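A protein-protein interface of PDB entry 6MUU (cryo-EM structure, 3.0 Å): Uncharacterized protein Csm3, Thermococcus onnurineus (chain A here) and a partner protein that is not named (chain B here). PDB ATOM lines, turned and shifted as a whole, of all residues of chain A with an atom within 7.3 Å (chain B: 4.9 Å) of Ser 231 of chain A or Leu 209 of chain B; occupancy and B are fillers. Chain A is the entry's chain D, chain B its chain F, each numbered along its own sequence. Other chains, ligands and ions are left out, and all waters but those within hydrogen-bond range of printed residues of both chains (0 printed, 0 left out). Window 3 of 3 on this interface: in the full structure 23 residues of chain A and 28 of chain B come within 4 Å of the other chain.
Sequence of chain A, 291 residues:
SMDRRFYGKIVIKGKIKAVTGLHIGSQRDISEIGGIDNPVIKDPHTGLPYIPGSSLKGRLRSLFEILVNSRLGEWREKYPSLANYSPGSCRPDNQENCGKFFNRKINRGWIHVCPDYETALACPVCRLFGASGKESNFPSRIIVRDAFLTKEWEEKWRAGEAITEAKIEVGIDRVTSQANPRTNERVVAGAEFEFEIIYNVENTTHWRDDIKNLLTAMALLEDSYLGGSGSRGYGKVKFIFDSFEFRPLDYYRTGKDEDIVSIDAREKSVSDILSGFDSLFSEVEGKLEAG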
ATOM      1  N   TYR A 225      19.431  25.898 -24.593  1.00  0.00           N
ATOM      2  CA  TYR A 225      18.645  26.040 -23.385  1.00  0.00           C
ATOM      3  C   TYR A 225      17.351  26.798 -23.662  1.00  0.00           C
ATOM      4  O   TYR A 225      17.075  27.228 -24.782  1.00  0.00           O
ATOM      5  CB  TYR A 225      19.481  26.738 -22.317  1.00  0.00           C
ATOM      6  CG  TYR A 225      19.950  28.131 -22.672  1.00  0.00           C
ATOM      7  CD1 TYR A 225      21.144  28.332 -23.352  1.00  0.00           C
ATOM      8  CD2 TYR A 225      19.226  29.247 -22.280  1.00  0.00           C
ATOM      9  CE1 TYR A 225      21.579  29.598 -23.663  1.00  0.00           C
ATOM     10  CE2 TYR A 225      19.654  30.515 -22.586  1.00  0.00           C
ATOM     11  CZ  TYR A 225      20.830  30.685 -23.276  1.00  0.00           C
ATOM     12  OH  TYR A 225      21.259  31.955 -23.577  1.00  0.00           O
ATOM     13  N   GLY A 228      17.263  32.076 -19.243  1.00  0.00           N
ATOM     14  CA  GLY A 228      17.803  32.223 -17.908  1.00  0.00           C
ATOM     15  C   GLY A 228      19.014  31.393 -17.548  1.00  0.00           C
ATOM     16  O   GLY A 228      18.859  30.380 -16.865  1.00  0.00           O
ATOM     17  N   SER A 229      20.190  31.757 -18.075  1.00  0.00           N
ATOM     18  CA  SER A 229      21.489  31.229 -17.629  1.00  0.00           C
ATOM     19  C   SER A 229      21.634  29.738 -17.921  1.00  0.00           C
ATOM     20  O   SER A 229      21.931  28.940 -17.036  1.00  0.00           O
ATOM     21  CB  SER A 229      21.730  31.520 -16.145  1.00  0.00           C
ATOM     22  OG  SER A 229      22.902  30.877 -15.686  1.00  0.00           O
ATOM     23  N   GLY A 230      21.422  29.371 -19.174  1.00  0.00           N
ATOM     24  CA  GLY A 230      21.537  27.991 -19.577  1.00  0.00           C
ATOM     25  C   GLY A 230      22.926  27.539 -19.931  1.00  0.00           C
ATOM     26  O   GLY A 230      23.120  26.370 -20.274  1.00  0.00           O
ATOM     27  N   SER A 231      23.913  28.432 -19.858  1.00  0.00           N
ATOM     28  CA  SER A 231      25.306  28.019 -19.943  1.00  0.00           C
ATOM     29  C   SER A 231      25.793  27.358 -18.664  1.00  0.00           C
ATOM     30  O   SER A 231      26.921  26.854 -18.635  1.00  0.00           O
ATOM     31  CB  SER A 231      26.195  29.216 -20.261  1.00  0.00           C
ATOM     32  OG  SER A 231      27.550  28.826 -20.293  1.00  0.00           O
ATOM     33  N   ARG A 232      24.973  27.356 -17.617  1.00  0.00           N
ATOM     34  CA  ARG A 232      25.308  26.814 -16.312  1.00  0.00           C
ATOM     35  C   ARG A 232      24.503  25.569 -16.006  1.00  0.00           C
ATOM     36  O   ARG A 232      24.713  24.949 -14.961  1.00  0.00           O
ATOM     37  CB  ARG A 232      25.061  27.855 -15.214  1.00  0.00           C
ATOM     38  CG  ARG A 232      26.134  28.920 -15.049  1.00  0.00           C
ATOM     39  CD  ARG A 232      26.033  29.978 -16.116  1.00  0.00           C
ATOM     40  NE  ARG A 232      27.013  31.029 -15.975  1.00  0.00           N
ATOM     41  CZ  ARG A 232      26.782  32.174 -15.363  1.00  0.00           C
ATOM     42  NH1 ARG A 232      27.750  33.064 -15.297  1.00  0.00           N
ATOM     43  NH2 ARG A 232      25.590  32.436 -14.848  1.00  0.00           N
ATOM     44  N   GLY A 233      23.580  25.198 -16.882  1.00  0.00           N
ATOM     45  CA  GLY A 233      22.754  24.027 -16.692  1.00  0.00           C
ATOM     46  C   GLY A 233      21.271  24.291 -16.686  1.00  0.00           C
ATOM     47  O   GLY A 233      20.497  23.331 -16.746  1.00  0.00           O
ATOM     48  N   TYR A 234      20.816  25.542 -16.668  1.00  0.00           N
ATOM     49  CA  TYR A 234      19.404  25.813 -16.419  1.00  0.00           C
ATOM     50  C   TYR A 234      18.509  25.596 -17.638  1.00  0.00           C
ATOM     51  O   TYR A 234      17.383  26.096 -17.653  1.00  0.00           O
ATOM     52  CB  TYR A 234      19.192  27.246 -15.926  1.00  0.00           C
ATOM     53  CG  TYR A 234      19.752  27.600 -14.566  1.00  0.00           C
ATOM     54  CD1 TYR A 234      20.268  26.638 -13.711  1.00  0.00           C
ATOM     55  CD2 TYR A 234      19.739  28.916 -14.135  1.00  0.00           C
ATOM     56  CE1 TYR A 234      20.780  26.987 -12.485  1.00  0.00           C
ATOM     57  CE2 TYR A 234      20.239  29.270 -12.913  1.00  0.00           C
ATOM     58  CZ  TYR A 234      20.758  28.307 -12.092  1.00  0.00           C
ATOM     59  OH  TYR A 234      21.254  28.678 -10.867  1.00  0.00           O
ATOM     60  N   GLY A 235      18.970  24.909 -18.671  1.00  0.00           N
ATOM     61  CA  GLY A 235      18.089  24.545 -19.755  1.00  0.00           C
ATOM     62  C   GLY A 235      17.857  23.056 -19.745  1.00  0.00           C
ATOM     63  O   GLY A 235      17.312  22.535 -18.767  1.00  0.00           O
ATOM     64  N   LYS B 118      31.725  24.771 -14.172  1.00  0.00           N
ATOM     65  CA  LYS B 118      32.166  25.800 -15.105  1.00  0.00           C
ATOM     66  C   LYS B 118      33.179  26.733 -14.456  1.00  0.00           C
ATOM     67  O   LYS B 118      34.039  27.291 -15.145  1.00  0.00           O
ATOM     68  CB  LYS B 118      30.964  26.591 -15.617  1.00  0.00           C
ATOM     69  CG  LYS B 118      31.259  27.518 -16.784  1.00  0.00           C
ATOM     70  CD  LYS B 118      30.016  28.242 -17.239  1.00  0.00           C
ATOM     71  CE  LYS B 118      30.288  29.021 -18.501  1.00  0.00           C
ATOM     72  NZ  LYS B 118      31.263  30.096 -18.268  1.00  0.00           N
ATOM     73  N   ILE B 121      36.894  25.354 -14.440  1.00  0.00           N
ATOM     74  CA  ILE B 121      37.556  25.472 -15.730  1.00  0.00           C
ATOM     75  C   ILE B 121      38.112  26.877 -15.918  1.00  0.00           C
ATOM     76  O   ILE B 121      39.228  27.040 -16.427  1.00  0.00           O
ATOM     77  CB  ILE B 121      36.583  25.084 -16.858  1.00  0.00           C
ATOM     78  CG1 ILE B 121      36.102  23.649 -16.679  1.00  0.00           C
ATOM     79  CG2 ILE B 121      37.249  25.192 -18.208  1.00  0.00           C
ATOM     80  CD1 ILE B 121      34.990  23.269 -17.629  1.00  0.00           C
ATOM     81  N   PRO B 205      34.105  35.507 -24.240  1.00  0.00           N
ATOM     82  CA  PRO B 205      34.101  34.252 -25.008  1.00  0.00           C
ATOM     83  C   PRO B 205      33.723  33.016 -24.208  1.00  0.00           C
ATOM     84  O   PRO B 205      33.823  31.909 -24.744  1.00  0.00           O
ATOM     85  CB  PRO B 205      35.555  34.133 -25.492  1.00  0.00           C
ATOM     86  CG  PRO B 205      36.098  35.500 -25.424  1.00  0.00           C
ATOM     87  CD  PRO B 205      35.436  36.132 -24.242  1.00  0.00           C
ATOM     88  N   MET B 206      33.317  33.153 -22.949  1.00  0.00           N
ATOM     89  CA  MET B 206      32.948  32.012 -22.126  1.00  0.00           C
ATOM     90  C   MET B 206      31.484  31.625 -22.269  1.00  0.00           C
ATOM     91  O   MET B 206      31.094  30.553 -21.794  1.00  0.00           O
ATOM     92  CB  MET B 206      33.259  32.308 -20.659  1.00  0.00           C
ATOM     93  CG  MET B 206      34.736  32.440 -20.360  1.00  0.00           C
ATOM     94  SD  MET B 206      35.624  30.925 -20.735  1.00  0.00           S
ATOM     95  CE  MET B 206      34.979  29.849 -19.466  1.00  0.00           C
ATOM     96  N   LYS B 207      30.673  32.458 -22.922  1.00  0.00           N
ATOM     97  CA  LYS B 207      29.253  32.182 -23.081  1.00  0.00           C
ATOM     98  C   LYS B 207      28.956  31.146 -24.151  1.00  0.00           C
ATOM     99  O   LYS B 207      27.810  30.701 -24.256  1.00  0.00           O
ATOM    100  CB  LYS B 207      28.499  33.472 -23.397  1.00  0.00           C
ATOM    101  CG  LYS B 207      28.832  34.108 -24.725  1.00  0.00           C
ATOM    102  CD  LYS B 207      28.076  35.414 -24.851  1.00  0.00           C
ATOM    103  CE  LYS B 207      28.365  36.114 -26.152  1.00  0.00           C
ATOM    104  NZ  LYS B 207      27.609  37.392 -26.231  1.00  0.00           N
ATOM    105  N   ALA B 208      29.945  30.760 -24.950  1.00  0.00           N
ATOM    106  CA  ALA B 208      29.746  29.672 -25.894  1.00  0.00           C
ATOM    107  C   ALA B 208      29.923  28.312 -25.238  1.00  0.00           C
ATOM    108  O   ALA B 208      29.337  27.326 -25.697  1.00  0.00           O
ATOM    109  CB  ALA B 208      30.712  29.816 -27.061  1.00  0.00           C
ATOM    110  N   LEU B 209      30.730  28.239 -24.186  1.00  0.00           N
ATOM    111  CA  LEU B 209      30.948  26.998 -23.451  1.00  0.00           C
ATOM    112  C   LEU B 209      29.763  26.779 -22.524  1.00  0.00           C
ATOM    113  O   LEU B 209      29.608  27.498 -21.533  1.00  0.00           O
ATOM    114  CB  LEU B 209      32.266  27.080 -22.685  1.00  0.00           C
ATOM    115  CG  LEU B 209      32.882  25.895 -21.934  1.00  0.00           C
ATOM    116  CD1 LEU B 209      32.359  25.738 -20.511  1.00  0.00           C
ATOM    117  CD2 LEU B 209      32.641  24.623 -22.720  1.00  0.00           C
ATOM    118  N   ILE B 210      28.927  25.791 -22.826  1.00  0.00           N
ATOM    119  CA  ILE B 210      27.783  25.477 -21.983  1.00  0.00           C
ATOM    120  C   ILE B 210      28.063  24.158 -21.278  1.00  0.00           C
ATOM    121  O   ILE B 210      28.614  23.223 -21.870  1.00  0.00           O
ATOM    122  CB  ILE B 210      26.450  25.467 -22.773  1.00  0.00           C
ATOM    123  CG1 ILE B 210      26.343  24.365 -23.830  1.00  0.00           C
ATOM    124  CG2 ILE B 210      26.242  26.800 -23.460  1.00  0.00           C
ATOM    125  CD1 ILE B 210      25.549  23.132 -23.388  1.00  0.00           C
ATOM    126  N   VAL B 211      27.742  24.112 -19.993  1.00  0.00           N
ATOM    127  CA  VAL B 211      27.795  22.892 -19.206  1.00  0.00           C
ATOM    128  C   VAL B 211      26.423  22.689 -18.592  1.00  0.00           C
ATOM    129  O   VAL B 211      25.664  23.643 -18.393  1.00  0.00           O
ATOM    130  CB  VAL B 211      28.890  22.938 -18.119  1.00  0.00           C
ATOM    131  CG1 VAL B 211      30.265  22.994 -18.749  1.00  0.00           C
ATOM    132  CG2 VAL B 211      28.690  24.139 -17.249  1.00  0.00           C
ATOM    133  N   ILE B 253      29.177  18.317 -21.318  1.00  0.00           N
ATOM    134  CA  ILE B 253      29.816  19.558 -21.737  1.00  0.00           C
ATOM    135  C   ILE B 253      29.715  19.658 -23.253  1.00  0.00           C
ATOM    136  O   ILE B 253      29.984  18.685 -23.970  1.00  0.00           O
ATOM    137  CB  ILE B 253      31.280  19.610 -21.264  1.00  0.00           C
ATOM    138  CG1 ILE B 253      31.339  19.552 -19.740  1.00  0.00           C
ATOM    139  CG2 ILE B 253      31.977  20.871 -21.744  1.00  0.00           C
ATOM    140  CD1 ILE B 253      32.731  19.347 -19.196  1.00  0.00           C
ATOM    141  N   HIS B 254      29.311  20.827 -23.741  1.00  0.00           N
ATOM    142  CA  HIS B 254      29.083  21.062 -25.157  1.00  0.00           C
ATOM    143  C   HIS B 254      29.540  22.473 -25.488  1.00  0.00           C
ATOM    144  O   HIS B 254      29.446  23.378 -24.656  1.00  0.00           O
ATOM    145  CB  HIS B 254      27.600  20.862 -25.509  1.00  0.00           C
ATOM    146  CG  HIS B 254      27.287  20.999 -26.965  1.00  0.00           C
ATOM    147  ND1 HIS B 254      26.978  22.208 -27.549  1.00  0.00           N
ATOM    148  CD2 HIS B 254      27.225  20.078 -27.955  1.00  0.00           C
ATOM    149  CE1 HIS B 254      26.745  22.028 -28.837  1.00  0.00           C
ATOM    150  NE2 HIS B 254      26.890  20.744 -29.109  1.00  0.00           N
ATOM    151  N   VAL B 255      30.051  22.656 -26.700  1.00  0.00           N
ATOM    152  CA  VAL B 255      30.576  23.941 -27.144  1.00  0.00           C
ATOM    153  C   VAL B 255      29.701  24.444 -28.281  1.00  0.00           C
ATOM    154  O   VAL B 255      29.379  23.687 -29.203  1.00  0.00           O
ATOM    155  CB  VAL B 255      32.048  23.829 -27.578  1.00  0.00           C
ATOM    156  CG1 VAL B 255      32.577  25.163 -28.097  1.00  0.00           C
ATOM    157  CG2 VAL B 255      32.894  23.343 -26.419  1.00  0.00           C
ATOM    158  N   PHE B 285      39.064  26.901 -29.954  1.00  0.00           N
ATOM    159  CA  PHE B 285      38.625  27.163 -28.557  1.00  0.00           C
ATOM    160  C   PHE B 285      38.588  25.854 -27.761  1.00  0.00           C
ATOM    161  O   PHE B 285      39.110  25.841 -26.634  1.00  0.00           O
ATOM    162  CB  PHE B 285      37.263  27.862 -28.546  1.00  0.00           C
ATOM    163  CG  PHE B 285      36.841  28.394 -27.200  1.00  0.00           C
ATOM    164  CD1 PHE B 285      37.302  29.619 -26.745  1.00  0.00           C
ATOM    165  CD2 PHE B 285      35.984  27.673 -26.386  1.00  0.00           C
ATOM    166  CE1 PHE B 285      36.914  30.108 -25.507  1.00  0.00           C
ATOM    167  CE2 PHE B 285      35.597  28.164 -25.150  1.00  0.00           C
ATOM    168  CZ  PHE B 285      36.064  29.379 -24.711  1.00  0.00           C
ATOM    169  N   LEU B 289      40.731  24.635 -24.511  1.00  0.00           N
ATOM    170  CA  LEU B 289      39.972  24.367 -23.294  1.00  0.00           C
ATOM    171  C   LEU B 289      40.595  23.231 -22.492  1.00  0.00           C
ATOM    172  O   LEU B 289      40.991  23.414 -21.337  1.00  0.00           O
ATOM    173  CB  LEU B 289      38.526  24.035 -23.658  1.00  0.00           C
ATOM    174  CG  LEU B 289      37.496  23.929 -22.540  1.00  0.00           C
ATOM    175  CD1 LEU B 289      37.254  25.302 -21.943  1.00  0.00           C
ATOM    176  CD2 LEU B 289      36.207  23.319 -23.055  1.00  0.00           C
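The side-chain hydroxyl of Ser 231 of chain A sits at hydrogen-bond distance from the backbone carbonyl oxygen of Leu 209 of chain B, at 2.7 Å.
The backbone carbonyl oxygen of Ser 231 of chain A lies within hydrogen-bond range of the backbone NH of Val 211 of chain B (3.2 Å).
The backbone NH (N) of Gly 233 of chain A is in hydrogen-bond range of the backbone carbonyl oxygen (O) of Val 211 of chain B (3.0 Å).
The side-chain hydroxyl (OG) of Ser 229 of chain A lies within hydrogen-bond range of the guanidinium group (NH2) of Arg 232 of chain A (3.2 Å).
The backbone NH (N) of Ile 210 of chain B is in hydrogen-bond range of the backbone carbonyl oxygen (O) of His 254 of chain B.
Among the printed residues, merely in contact across the chains: Ser 231 of chain A with Lys 118 of chain B, Arg 232 of chain A with Val 211 of chain B and Ser 231 of chain A with Ile 210 of chain B.
Ser 231 of chain A touches just these residues of chain B: Lys 118, Leu 209, Ile 210 and Val 211.
Leu 209 of chain B touches just one residue of chain A: Ser 231.
Of the printed residues of chain A, Val 211 of chain B touches Ser 231 (3.2 Å), Arg 232 (3.3 Å) and Gly 233 (3.0 Å).
Printed residues of chain A within 4 Å of Ile 210 of chain B: Ser 231.
The nearest residue of chain A that does not touch Leu 209 of chain B is Arg 232 of chain A (6.1 Å).
The nearest printed residue of chain B that does not touch Gly 233 of chain A is Ile 210 of chain B (6.4 Å).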
